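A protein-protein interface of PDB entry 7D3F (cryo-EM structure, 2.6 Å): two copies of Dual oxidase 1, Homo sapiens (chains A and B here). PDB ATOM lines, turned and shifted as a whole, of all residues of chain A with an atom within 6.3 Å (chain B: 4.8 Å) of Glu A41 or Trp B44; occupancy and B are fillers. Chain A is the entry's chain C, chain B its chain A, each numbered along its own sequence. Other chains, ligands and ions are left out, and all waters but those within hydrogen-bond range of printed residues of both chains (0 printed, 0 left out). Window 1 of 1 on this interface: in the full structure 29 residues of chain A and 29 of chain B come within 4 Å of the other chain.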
ATOM      1  N   TYR A  36      13.687   8.237  20.328  1.00  0.00           N
ATOM      2  CA  TYR A  36      12.923   8.492  19.109  1.00  0.00           C
ATOM      3  C   TYR A  36      11.703   9.372  19.349  1.00  0.00           C
ATOM      4  O   TYR A  36      10.738   9.322  18.582  1.00  0.00           O
ATOM      5  CB  TYR A  36      12.498   7.182  18.437  1.00  0.00           C
ATOM      6  CG  TYR A  36      13.634   6.212  18.212  1.00  0.00           C
ATOM      7  CD1 TYR A  36      14.668   6.514  17.336  1.00  0.00           C
ATOM      8  CD2 TYR A  36      13.670   4.992  18.873  1.00  0.00           C
ATOM      9  CE1 TYR A  36      15.708   5.627  17.128  1.00  0.00           C
ATOM     10  CE2 TYR A  36      14.704   4.100  18.670  1.00  0.00           C
ATOM     11  CZ  TYR A  36      15.720   4.423  17.798  1.00  0.00           C
ATOM     12  OH  TYR A  36      16.750   3.535  17.596  1.00  0.00           O
ATOM     13  N   ASN A  37      11.715  10.178  20.413  1.00  0.00           N
ATOM     14  CA  ASN A  37      10.632  11.134  20.614  1.00  0.00           C
ATOM     15  C   ASN A  37      10.747  12.297  19.636  1.00  0.00           C
ATOM     16  O   ASN A  37       9.743  12.736  19.063  1.00  0.00           O
ATOM     17  CB  ASN A  37      10.636  11.624  22.061  1.00  0.00           C
ATOM     18  CG  ASN A  37       9.384  12.410  22.424  1.00  0.00           C
ATOM     19  OD1 ASN A  37       8.997  13.349  21.729  1.00  0.00           O
ATOM     20  ND2 ASN A  37       8.748  12.026  23.524  1.00  0.00           N
ATOM     21  N   ASN A  38      11.960  12.801  19.427  1.00  0.00           N
ATOM     22  CA  ASN A  38      12.209  13.838  18.437  1.00  0.00           C
ATOM     23  C   ASN A  38      12.623  13.197  17.120  1.00  0.00           C
ATOM     24  O   ASN A  38      13.300  12.164  17.105  1.00  0.00           O
ATOM     25  CB  ASN A  38      13.291  14.804  18.921  1.00  0.00           C
ATOM     26  CG  ASN A  38      13.450  16.006  18.010  1.00  0.00           C
ATOM     27  OD1 ASN A  38      14.205  15.968  17.039  1.00  0.00           O
ATOM     28  ND2 ASN A  38      12.739  17.082  18.324  1.00  0.00           N
ATOM     29  N   LEU A  39      12.205  13.814  16.011  1.00  0.00           N
ATOM     30  CA  LEU A  39      12.415  13.206  14.700  1.00  0.00           C
ATOM     31  C   LEU A  39      13.897  13.070  14.369  1.00  0.00           C
ATOM     32  O   LEU A  39      14.335  12.027  13.869  1.00  0.00           O
ATOM     33  CB  LEU A  39      11.699  14.021  13.622  1.00  0.00           C
ATOM     34  CG  LEU A  39      11.839  13.490  12.195  1.00  0.00           C
ATOM     35  CD1 LEU A  39      11.349  12.053  12.106  1.00  0.00           C
ATOM     36  CD2 LEU A  39      11.089  14.377  11.215  1.00  0.00           C
ATOM     37  N   MET A  40      14.688  14.110  14.641  1.00  0.00           N
ATOM     38  CA  MET A  40      16.091  14.118  14.257  1.00  0.00           C
ATOM     39  C   MET A  40      17.056  13.997  15.427  1.00  0.00           C
ATOM     40  O   MET A  40      18.222  13.651  15.207  1.00  0.00           O
ATOM     41  CB  MET A  40      16.419  15.396  13.472  1.00  0.00           C
ATOM     42  CG  MET A  40      15.578  15.574  12.219  1.00  0.00           C
ATOM     43  SD  MET A  40      15.737  14.193  11.072  1.00  0.00           S
ATOM     44  CE  MET A  40      17.490  14.254  10.716  1.00  0.00           C
ATOM     45  N   GLU A  41      16.611  14.269  16.648  1.00  0.00           N
ATOM     46  CA  GLU A  41      17.437  14.134  17.846  1.00  0.00           C
ATOM     47  C   GLU A  41      16.853  12.991  18.672  1.00  0.00           C
ATOM     48  O   GLU A  41      16.020  13.202  19.555  1.00  0.00           O
ATOM     49  CB  GLU A  41      17.483  15.440  18.632  1.00  0.00           C
ATOM     50  CG  GLU A  41      18.146  16.591  17.890  1.00  0.00           C
ATOM     51  CD  GLU A  41      19.650  16.425  17.774  1.00  0.00           C
ATOM     52  OE1 GLU A  41      20.225  15.623  18.539  1.00  0.00           O
ATOM     53  OE2 GLU A  41      20.259  17.099  16.916  1.00  0.00           O
ATOM     54  N   HIS A  42      17.306  11.770  18.379  1.00  0.00           N
ATOM     55  CA  HIS A  42      16.744  10.586  19.016  1.00  0.00           C
ATOM     56  C   HIS A  42      17.127  10.466  20.485  1.00  0.00           C
ATOM     57  O   HIS A  42      16.426   9.783  21.238  1.00  0.00           O
ATOM     58  CB  HIS A  42      17.181   9.332  18.257  1.00  0.00           C
ATOM     59  CG  HIS A  42      16.743   9.312  16.825  1.00  0.00           C
ATOM     60  ND1 HIS A  42      17.397   8.581  15.857  1.00  0.00           N
ATOM     61  CD2 HIS A  42      15.715   9.932  16.199  1.00  0.00           C
ATOM     62  CE1 HIS A  42      16.791   8.753  14.695  1.00  0.00           C
ATOM     63  NE2 HIS A  42      15.767   9.568  14.876  1.00  0.00           N
ATOM     64  N   ARG A  43      18.214  11.107  20.909  1.00  0.00           N
ATOM     65  CA  ARG A  43      18.668  11.021  22.291  1.00  0.00           C
ATOM     66  C   ARG A  43      18.087  12.108  23.185  1.00  0.00           C
ATOM     67  O   ARG A  43      18.385  12.124  24.384  1.00  0.00           O
ATOM     68  CB  ARG A  43      20.198  11.075  22.350  1.00  0.00           C
ATOM     69  CG  ARG A  43      20.878   9.776  21.956  1.00  0.00           C
ATOM     70  CD  ARG A  43      22.387   9.864  22.128  1.00  0.00           C
ATOM     71  NE  ARG A  43      22.764  10.280  23.476  1.00  0.00           N
ATOM     72  CZ  ARG A  43      22.919   9.447  24.501  1.00  0.00           C
ATOM     73  NH1 ARG A  43      22.724   8.146  24.338  1.00  0.00           N
ATOM     74  NH2 ARG A  43      23.266   9.917  25.691  1.00  0.00           N
ATOM     75  N   TRP A  44      17.274  13.012  22.644  1.00  0.00           N
ATOM     76  CA  TRP A  44      16.670  14.053  23.464  1.00  0.00           C
ATOM     77  C   TRP A  44      15.667  13.446  24.436  1.00  0.00           C
ATOM     78  O   TRP A  44      14.795  12.667  24.040  1.00  0.00           O
ATOM     79  CB  TRP A  44      15.989  15.099  22.583  1.00  0.00           C
ATOM     80  CG  TRP A  44      16.918  16.164  22.096  1.00  0.00           C
ATOM     81  CD1 TRP A  44      18.257  16.255  22.337  1.00  0.00           C
ATOM     82  CD2 TRP A  44      16.577  17.299  21.293  1.00  0.00           C
ATOM     83  NE1 TRP A  44      18.773  17.373  21.728  1.00  0.00           N
ATOM     84  CE2 TRP A  44      17.761  18.032  21.081  1.00  0.00           C
ATOM     85  CE3 TRP A  44      15.385  17.764  20.726  1.00  0.00           C
ATOM     86  CZ2 TRP A  44      17.789  19.204  20.330  1.00  0.00           C
ATOM     87  CZ3 TRP A  44      15.415  18.929  19.981  1.00  0.00           C
ATOM     88  CH2 TRP A  44      16.609  19.635  19.789  1.00  0.00           C
ATOM     89  N   GLY A  45      15.801  13.797  25.714  1.00  0.00           N
ATOM     90  CA  GLY A  45      14.901  13.297  26.732  1.00  0.00           C
ATOM     91  C   GLY A  45      15.030  11.823  27.038  1.00  0.00           C
ATOM     92  O   GLY A  45      14.216  11.290  27.798  1.00  0.00           O
ATOM     93  N   GLN A  52      21.133  19.798  29.934  1.00  0.00           N
ATOM     94  CA  GLN A  52      21.412  21.078  29.307  1.00  0.00           C
ATOM     95  C   GLN A  52      22.071  22.027  30.304  1.00  0.00           C
ATOM     96  O   GLN A  52      22.107  21.783  31.513  1.00  0.00           O
ATOM     97  CB  GLN A  52      20.129  21.695  28.752  1.00  0.00           C
ATOM     98  CG  GLN A  52      19.822  21.309  27.315  1.00  0.00           C
ATOM     99  CD  GLN A  52      20.694  22.047  26.317  1.00  0.00           C
ATOM    100  OE1 GLN A  52      21.198  23.132  26.602  1.00  0.00           O
ATOM    101  NE2 GLN A  52      20.876  21.459  25.140  1.00  0.00           N
ATOM    102  N   TRP A 172      11.601  13.375  29.552  1.00  0.00           N
ATOM    103  CA  TRP A 172      10.223  13.670  29.193  1.00  0.00           C
ATOM    104  C   TRP A 172       9.309  13.546  30.404  1.00  0.00           C
ATOM    105  O   TRP A 172       9.581  12.799  31.347  1.00  0.00           O
ATOM    106  CB  TRP A 172       9.745  12.725  28.092  1.00  0.00           C
ATOM    107  CG  TRP A 172      10.629  12.711  26.895  1.00  0.00           C
ATOM    108  CD1 TRP A 172      11.491  11.724  26.521  1.00  0.00           C
ATOM    109  CD2 TRP A 172      10.748  13.742  25.910  1.00  0.00           C
ATOM    110  NE1 TRP A 172      12.137  12.073  25.360  1.00  0.00           N
ATOM    111  CE2 TRP A 172      11.698  13.309  24.966  1.00  0.00           C
ATOM    112  CE3 TRP A 172      10.142  14.988  25.734  1.00  0.00           C
ATOM    113  CZ2 TRP A 172      12.057  14.080  23.864  1.00  0.00           C
ATOM    114  CZ3 TRP A 172      10.499  15.747  24.641  1.00  0.00           C
ATOM    115  CH2 TRP A 172      11.442  15.288  23.716  1.00  0.00           C
ATOM    116  N   PRO A 312       9.413  20.725  17.022  1.00  0.00           N
ATOM    117  CA  PRO A 312      10.433  19.683  16.821  1.00  0.00           C
ATOM    118  C   PRO A 312      11.860  20.173  16.995  1.00  0.00           C
ATOM    119  O   PRO A 312      12.744  19.355  17.278  1.00  0.00           O
ATOM    120  CB  PRO A 312      10.184  19.215  15.378  1.00  0.00           C
ATOM    121  CG  PRO A 312       8.802  19.694  15.041  1.00  0.00           C
ATOM    122  CD  PRO A 312       8.617  20.963  15.807  1.00  0.00           C
ATOM    123  N   PHE A 313      12.116  21.471  16.836  1.00  0.00           N
ATOM    124  CA  PHE A 313      13.468  22.010  16.861  1.00  0.00           C
ATOM    125  C   PHE A 313      13.848  22.599  18.213  1.00  0.00           C
ATOM    126  O   PHE A 313      14.926  23.188  18.338  1.00  0.00           O
ATOM    127  CB  PHE A 313      13.631  23.066  15.768  1.00  0.00           C
ATOM    128  CG  PHE A 313      13.189  22.604  14.411  1.00  0.00           C
ATOM    129  CD1 PHE A 313      14.026  21.835  13.620  1.00  0.00           C
ATOM    130  CD2 PHE A 313      11.936  22.938  13.926  1.00  0.00           C
ATOM    131  CE1 PHE A 313      13.621  21.408  12.371  1.00  0.00           C
ATOM    132  CE2 PHE A 313      11.525  22.513  12.676  1.00  0.00           C
ATOM    133  CZ  PHE A 313      12.369  21.746  11.899  1.00  0.00           C
ATOM    134  N   LEU A 314      12.996  22.454  19.222  1.00  0.00           N
ATOM    135  CA  LEU A 314      13.260  22.979  20.554  1.00  0.00           C
ATOM    136  C   LEU A 314      13.841  21.877  21.427  1.00  0.00           C
ATOM    137  O   LEU A 314      13.268  20.786  21.518  1.00  0.00           O
ATOM    138  CB  LEU A 314      11.982  23.536  21.182  1.00  0.00           C
ATOM    139  CG  LEU A 314      12.120  24.157  22.573  1.00  0.00           C
ATOM    140  CD1 LEU A 314      13.037  25.370  22.530  1.00  0.00           C
ATOM    141  CD2 LEU A 314      10.755  24.531  23.129  1.00  0.00           C
ATOM    142  N   ASP A 315      14.975  22.160  22.059  1.00  0.00           N
ATOM    143  CA  ASP A 315      15.620  21.177  22.921  1.00  0.00           C
ATOM    144  C   ASP A 315      14.930  21.155  24.280  1.00  0.00           C
ATOM    145  O   ASP A 315      14.955  22.166  24.991  1.00  0.00           O
ATOM    146  CB  ASP A 315      17.101  21.498  23.083  1.00  0.00           C
ATOM    147  CG  ASP A 315      17.876  20.374  23.749  1.00  0.00           C
ATOM    148  OD1 ASP A 315      17.269  19.334  24.078  1.00  0.00           O
ATOM    149  OD2 ASP A 315      19.100  20.530  23.939  1.00  0.00           O
ATOM    150  N   GLY B  34      32.082  26.002  11.995  1.00  0.00           N
ATOM    151  CA  GLY B  34      30.780  26.011  12.625  1.00  0.00           C
ATOM    152  C   GLY B  34      30.686  25.230  13.916  1.00  0.00           C
ATOM    153  O   GLY B  34      29.590  25.139  14.485  1.00  0.00           O
ATOM    154  N   ASN B  37      29.390  26.435  18.148  1.00  0.00           N
ATOM    155  CA  ASN B  37      28.527  27.610  18.104  1.00  0.00           C
ATOM    156  C   ASN B  37      27.435  27.519  19.163  1.00  0.00           C
ATOM    157  O   ASN B  37      27.136  28.508  19.842  1.00  0.00           O
ATOM    158  CB  ASN B  37      27.931  27.764  16.705  1.00  0.00           C
ATOM    159  CG  ASN B  37      27.239  29.103  16.501  1.00  0.00           C
ATOM    160  OD1 ASN B  37      26.393  29.513  17.296  1.00  0.00           O
ATOM    161  ND2 ASN B  37      27.597  29.791  15.423  1.00  0.00           N
ATOM    162  N   ASN B  38      26.836  26.341  19.323  1.00  0.00           N
ATOM    163  CA  ASN B  38      25.858  26.107  20.374  1.00  0.00           C
ATOM    164  C   ASN B  38      26.554  25.534  21.601  1.00  0.00           C
ATOM    165  O   ASN B  38      27.516  24.769  21.483  1.00  0.00           O
ATOM    166  CB  ASN B  38      24.761  25.154  19.893  1.00  0.00           C
ATOM    167  CG  ASN B  38      23.623  25.027  20.885  1.00  0.00           C
ATOM    168  OD1 ASN B  38      23.665  24.197  21.793  1.00  0.00           O
ATOM    169  ND2 ASN B  38      22.596  25.852  20.716  1.00  0.00           N
ATOM    170  N   GLU B  41      25.149  21.631  21.864  1.00  0.00           N
ATOM    171  CA  GLU B  41      25.120  20.894  20.603  1.00  0.00           C
ATOM    172  C   GLU B  41      26.248  21.441  19.731  1.00  0.00           C
ATOM    173  O   GLU B  41      26.050  22.357  18.932  1.00  0.00           O
ATOM    174  CB  GLU B  41      23.761  21.023  19.923  1.00  0.00           C
ATOM    175  CG  GLU B  41      22.611  20.405  20.705  1.00  0.00           C
ATOM    176  CD  GLU B  41      22.646  18.888  20.700  1.00  0.00           C
ATOM    177  OE1 GLU B  41      23.333  18.308  19.833  1.00  0.00           O
ATOM    178  OE2 GLU B  41      21.985  18.275  21.565  1.00  0.00           O
ATOM    179  N   HIS B  42      27.440  20.861  19.891  1.00  0.00           N
ATOM    180  CA  HIS B  42      28.621  21.367  19.203  1.00  0.00           C
ATOM    181  C   HIS B  42      28.595  21.093  17.706  1.00  0.00           C
ATOM    182  O   HIS B  42      29.280  21.790  16.951  1.00  0.00           O
ATOM    183  CB  HIS B  42      29.881  20.763  19.823  1.00  0.00           C
ATOM    184  CG  HIS B  42      30.049  21.080  21.276  1.00  0.00           C
ATOM    185  ND1 HIS B  42      30.786  20.291  22.131  1.00  0.00           N
ATOM    186  CD2 HIS B  42      29.575  22.104  22.025  1.00  0.00           C
ATOM    187  CE1 HIS B  42      30.758  20.813  23.345  1.00  0.00           C
ATOM    188  NE2 HIS B  42      30.030  21.914  23.307  1.00  0.00           N
ATOM    189  N   ARG B  43      27.826  20.103  17.257  1.00  0.00           N
ATOM    190  CA  ARG B  43      27.766  19.754  15.844  1.00  0.00           C
ATOM    191  C   ARG B  43      26.673  20.497  15.085  1.00  0.00           C
ATOM    192  O   ARG B  43      26.543  20.298  13.874  1.00  0.00           O
ATOM    193  CB  ARG B  43      27.565  18.244  15.678  1.00  0.00           C
ATOM    194  CG  ARG B  43      28.821  17.424  15.915  1.00  0.00           C
ATOM    195  CD  ARG B  43      28.580  15.948  15.641  1.00  0.00           C
ATOM    196  NE  ARG B  43      28.033  15.717  14.306  1.00  0.00           N
ATOM    197  CZ  ARG B  43      28.769  15.573  13.209  1.00  0.00           C
ATOM    198  NH1 ARG B  43      30.092  15.639  13.280  1.00  0.00           N
ATOM    199  NH2 ARG B  43      28.181  15.364  12.038  1.00  0.00           N
ATOM    200  N   TRP B  44      25.892  21.339  15.756  1.00  0.00           N
ATOM    201  CA  TRP B  44      24.853  22.095  15.068  1.00  0.00           C
ATOM    202  C   TRP B  44      25.477  23.117  14.126  1.00  0.00           C
ATOM    203  O   TRP B  44      26.361  23.883  14.521  1.00  0.00           O
ATOM    204  CB  TRP B  44      23.943  22.792  16.079  1.00  0.00           C
ATOM    205  CG  TRP B  44      22.833  21.924  16.580  1.00  0.00           C
ATOM    206  CD1 TRP B  44      22.599  20.622  16.248  1.00  0.00           C
ATOM    207  CD2 TRP B  44      21.798  22.298  17.495  1.00  0.00           C
ATOM    208  NE1 TRP B  44      21.486  20.158  16.905  1.00  0.00           N
ATOM    209  CE2 TRP B  44      20.976  21.168  17.678  1.00  0.00           C
ATOM    210  CE3 TRP B  44      21.490  23.475  18.185  1.00  0.00           C
ATOM    211  CZ2 TRP B  44      19.864  21.182  18.517  1.00  0.00           C
ATOM    212  CZ3 TRP B  44      20.386  23.487  19.018  1.00  0.00           C
ATOM    213  CH2 TRP B  44      19.587  22.348  19.177  1.00  0.00           C
ATOM    214  N   GLY B  45      25.021  23.117  12.875  1.00  0.00           N
ATOM    215  CA  GLY B  45      25.525  24.049  11.888  1.00  0.00           C
ATOM    216  C   GLY B  45      26.953  23.818  11.454  1.00  0.00           C
ATOM    217  O   GLY B  45      27.501  24.639  10.715  1.00  0.00           O
ATOM    218  N   SER B  46      27.573  22.723  11.884  1.00  0.00           N
ATOM    219  CA  SER B  46      28.959  22.463  11.540  1.00  0.00           C
ATOM    220  C   SER B  46      29.057  21.781  10.180  1.00  0.00           C
ATOM    221  O   SER B  46      28.084  21.230   9.656  1.00  0.00           O
ATOM    222  CB  SER B  46      29.626  21.599  12.609  1.00  0.00           C
ATOM    223  OG  SER B  46      29.001  20.330  12.690  1.00  0.00           O
ATOM    224  N   ARG B  50      24.388  16.467   9.688  1.00  0.00           N
ATOM    225  CA  ARG B  50      23.215  16.044   8.940  1.00  0.00           C
ATOM    226  C   ARG B  50      22.197  17.178   8.844  1.00  0.00           C
ATOM    227  O   ARG B  50      22.188  18.118   9.644  1.00  0.00           O
ATOM    228  CB  ARG B  50      22.573  14.814   9.585  1.00  0.00           C
ATOM    229  CG  ARG B  50      21.504  15.123  10.626  1.00  0.00           C
ATOM    230  CD  ARG B  50      22.105  15.437  11.986  1.00  0.00           C
ATOM    231  NE  ARG B  50      21.791  16.792  12.430  1.00  0.00           N
ATOM    232  CZ  ARG B  50      20.648  17.146  13.010  1.00  0.00           C
ATOM    233  NH1 ARG B  50      19.697  16.245  13.215  1.00  0.00           N
ATOM    234  NH2 ARG B  50      20.454  18.403  13.382  1.00  0.00           N
ATOM    235  N   TRP B 172      25.542  27.557   9.332  1.00  0.00           N
ATOM    236  CA  TRP B 172      25.403  28.922   9.813  1.00  0.00           C
ATOM    237  C   TRP B 172      25.522  29.916   8.666  1.00  0.00           C
ATOM    238  O   TRP B 172      26.167  29.656   7.647  1.00  0.00           O
ATOM    239  CB  TRP B 172      26.469  29.227  10.865  1.00  0.00           C
ATOM    240  CG  TRP B 172      26.490  28.252  11.990  1.00  0.00           C
ATOM    241  CD1 TRP B 172      27.420  27.280  12.218  1.00  0.00           C
ATOM    242  CD2 TRP B 172      25.530  28.144  13.044  1.00  0.00           C
ATOM    243  NE1 TRP B 172      27.100  26.577  13.354  1.00  0.00           N
ATOM    244  CE2 TRP B 172      25.942  27.088  13.879  1.00  0.00           C
ATOM    245  CE3 TRP B 172      24.362  28.840  13.364  1.00  0.00           C
ATOM    246  CZ2 TRP B 172      25.226  26.710  15.010  1.00  0.00           C
ATOM    247  CZ3 TRP B 172      23.656  28.464  14.487  1.00  0.00           C
ATOM    248  CH2 TRP B 172      24.093  27.414  15.301  1.00  0.00           C
ATOM    249  N   PRO B 312      19.384  29.366  22.549  1.00  0.00           N
ATOM    250  CA  PRO B 312      20.339  28.245  22.590  1.00  0.00           C
ATOM    251  C   PRO B 312      19.704  26.885  22.353  1.00  0.00           C
ATOM    252  O   PRO B 312      20.412  25.958  21.940  1.00  0.00           O
ATOM    253  CB  PRO B 312      20.934  28.336  24.003  1.00  0.00           C
ATOM    254  CG  PRO B 312      20.616  29.723  24.477  1.00  0.00           C
ATOM    255  CD  PRO B 312      19.316  30.081  23.833  1.00  0.00           C
ATOM    256  N   PHE B 313      18.404  26.734  22.597  1.00  0.00           N
ATOM    257  CA  PHE B 313      17.737  25.442  22.519  1.00  0.00           C
ATOM    258  C   PHE B 313      17.015  25.225  21.195  1.00  0.00           C
ATOM    259  O   PHE B 313      16.316  24.220  21.041  1.00  0.00           O
ATOM    260  CB  PHE B 313      16.755  25.289  23.680  1.00  0.00           C
ATOM    261  CG  PHE B 313      17.356  25.580  25.023  1.00  0.00           C
ATOM    262  CD1 PHE B 313      18.094  24.616  25.689  1.00  0.00           C
ATOM    263  CD2 PHE B 313      17.185  26.817  25.620  1.00  0.00           C
ATOM    264  CE1 PHE B 313      18.650  24.882  26.925  1.00  0.00           C
ATOM    265  CE2 PHE B 313      17.740  27.089  26.857  1.00  0.00           C
ATOM    266  CZ  PHE B 313      18.473  26.119  27.508  1.00  0.00           C
ATOM    267  N   LEU B 314      17.170  26.137  20.240  1.00  0.00           N
ATOM    268  CA  LEU B 314      16.523  26.027  18.940  1.00  0.00           C
ATOM    269  C   LEU B 314      17.499  25.424  17.939  1.00  0.00           C
ATOM    270  O   LEU B 314      18.628  25.905  17.801  1.00  0.00           O
ATOM    271  CB  LEU B 314      16.043  27.395  18.454  1.00  0.00           C
ATOM    272  CG  LEU B 314      15.310  27.423  17.112  1.00  0.00           C
ATOM    273  CD1 LEU B 314      14.025  26.613  17.187  1.00  0.00           C
ATOM    274  CD2 LEU B 314      15.023  28.855  16.690  1.00  0.00           C
ATOM    275  N   ASP B 315      17.065  24.373  17.251  1.00  0.00           N
ATOM    276  CA  ASP B 315      17.916  23.716  16.267  1.00  0.00           C
ATOM    277  C   ASP B 315      17.900  24.509  14.965  1.00  0.00           C
ATOM    278  O   ASP B 315      16.842  24.630  14.339  1.00  0.00           O
ATOM    279  CB  ASP B 315      17.447  22.287  16.022  1.00  0.00           C
ATOM    280  CG  ASP B 315      18.441  21.472  15.212  1.00  0.00           C
ATOM    281  OD1 ASP B 315      19.505  22.013  14.841  1.00  0.00           O
ATOM    282  OD2 ASP B 315      18.160  20.285  14.949  1.00  0.00           O
ATOM    283  N   PRO B 316      19.033  25.059  14.527  1.00  0.00           N
ATOM    284  CA  PRO B 316      19.071  25.844  13.281  1.00  0.00           C
ATOM    285  C   PRO B 316      19.509  25.064  12.047  1.00  0.00           C
ATOM    286  O   PRO B 316      19.722  25.693  11.005  1.00  0.00           O
ATOM    287  CB  PRO B 316      20.111  26.913  13.624  1.00  0.00           C
ATOM    288  CG  PRO B 316      21.095  26.158  14.459  1.00  0.00           C
ATOM    289  CD  PRO B 316      20.315  25.131  15.249  1.00  0.00           C
ATOM    290  N   SER B 317      19.663  23.744  12.144  1.00  0.00           N
ATOM    291  CA  SER B 317      20.192  22.965  11.034  1.00  0.00           C
ATOM    292  C   SER B 317      19.310  23.109   9.802  1.00  0.00           C
ATOM    293  O   SER B 317      18.079  23.148   9.896  1.00  0.00           O
ATOM    294  CB  SER B 317      20.310  21.492  11.429  1.00  0.00           C
ATOM    295  OG  SER B 317      21.127  21.337  12.577  1.00  0.00           O
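Glu A41 touches Trp B44, and with the chains exchanged Trp A44 touches Glu B41.
Phe A313 touches its own counterpart, Phe B313.
Phe A313 touches Leu B314, and with the chains exchanged Leu A314 touches Phe B313.
Phe A313 touches Asp B315, and with the chains exchanged Asp A315 touches Phe B313.
O of Phe B313 lies within hydrogen-bond range of N of Asp A315 (2.7 Å).
The backbone carbonyl oxygen of Phe B313 lies close to the backbone carbonyl oxygen of Phe A313 (3.2 Å).
The backbone NH (N) of Asp B315 sits at hydrogen-bond distance from the backbone carbonyl oxygen (O) of Phe A313.
NE1 of Trp B44 is in hydrogen-bond range of OE2 of Glu A41.
The side-chain carboxylate (OE2) of Glu A41 is in salt-bridge range of the guanidinium group (NH2) of Arg B50 (3.8 Å).
NE1 of Trp A44 is in hydrogen-bond range of OE2 of Glu B41 (3.3 Å).
N of Glu A41 sits at hydrogen-bond distance from OD1 of Asn A38 (3.0 Å).
The backbone NH (N) of Met A40 sits at hydrogen-bond distance from the side-chain amide oxygen (OD1) of Asn A38, 3.1 Å away.
The guanidinium group (NH2) of Arg B50 is in salt-bridge range of the side-chain carboxylate (OD2) of Asp B315, at 3.4 Å.
NE1 of Trp A172 is in hydrogen-bond range of O of Trp A44.
OD1 of Asp B315 lies close to NE1 of Trp B44.
The indole nitrogen of Trp B172 sits at hydrogen-bond distance from the backbone carbonyl oxygen of Trp B44 (3.0 Å).
Of the 16 printed residues of chain A, 7 touch a printed residue of chain B.
Of the 17 printed residues of chain B, 6 touch a printed residue of chain A.
Hydrophobic or aromatic side chains of chain B that line the printed part of chain A: Trp B44, Phe B313 and Leu B314.
Among the printed residues, 11 pairs touch across the chains.
Among the printed residues, Asp or Glu carboxylates within 4 Å of a Lys or Arg side-chain nitrogen of the other chain: Glu A41 with Arg B50 (3.8 Å).
Of the printed residues of chain B, Glu A41 touches Trp B44 and Arg B50.
Of chain A, only Glu A41 (3.3 Å) and Trp A44 (3.4 Å) come within 4 Å of Trp B44.
Of the printed residues of chain B, Met A40 touches Arg B50.
Of the printed residues of chain B, Phe A313 touches Phe B313 (3.2 Å), Leu B314 (3.3 Å) and Asp B315 (2.7 Å).
Of the printed residues of chain B, Trp A44 touches Glu B41 and Trp B44.
Of the printed residues of chain A, Phe B313 touches Gln A52 (3.1 Å), Phe A313 (3.2 Å), Leu A314 (3.3 Å) and Asp A315 (2.7 Å).
Of the printed residues of chain A, Leu B314 touches Phe A313 (3.3 Å).
The nearest printed residue of chain B that does not touch Glu A41 is Asp B315 (4.3 Å).
The nearest printed residue of chain A that does not touch Arg B50 is Asn A38 (6.7 Å).
Among the printed residues, pairs that only touch across the chains: Gln A52 with Phe B313, Phe A313 with Leu B314, Leu A314 with Phe B313, Trp A44 with Trp B44 and Met A40 with Arg B50.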
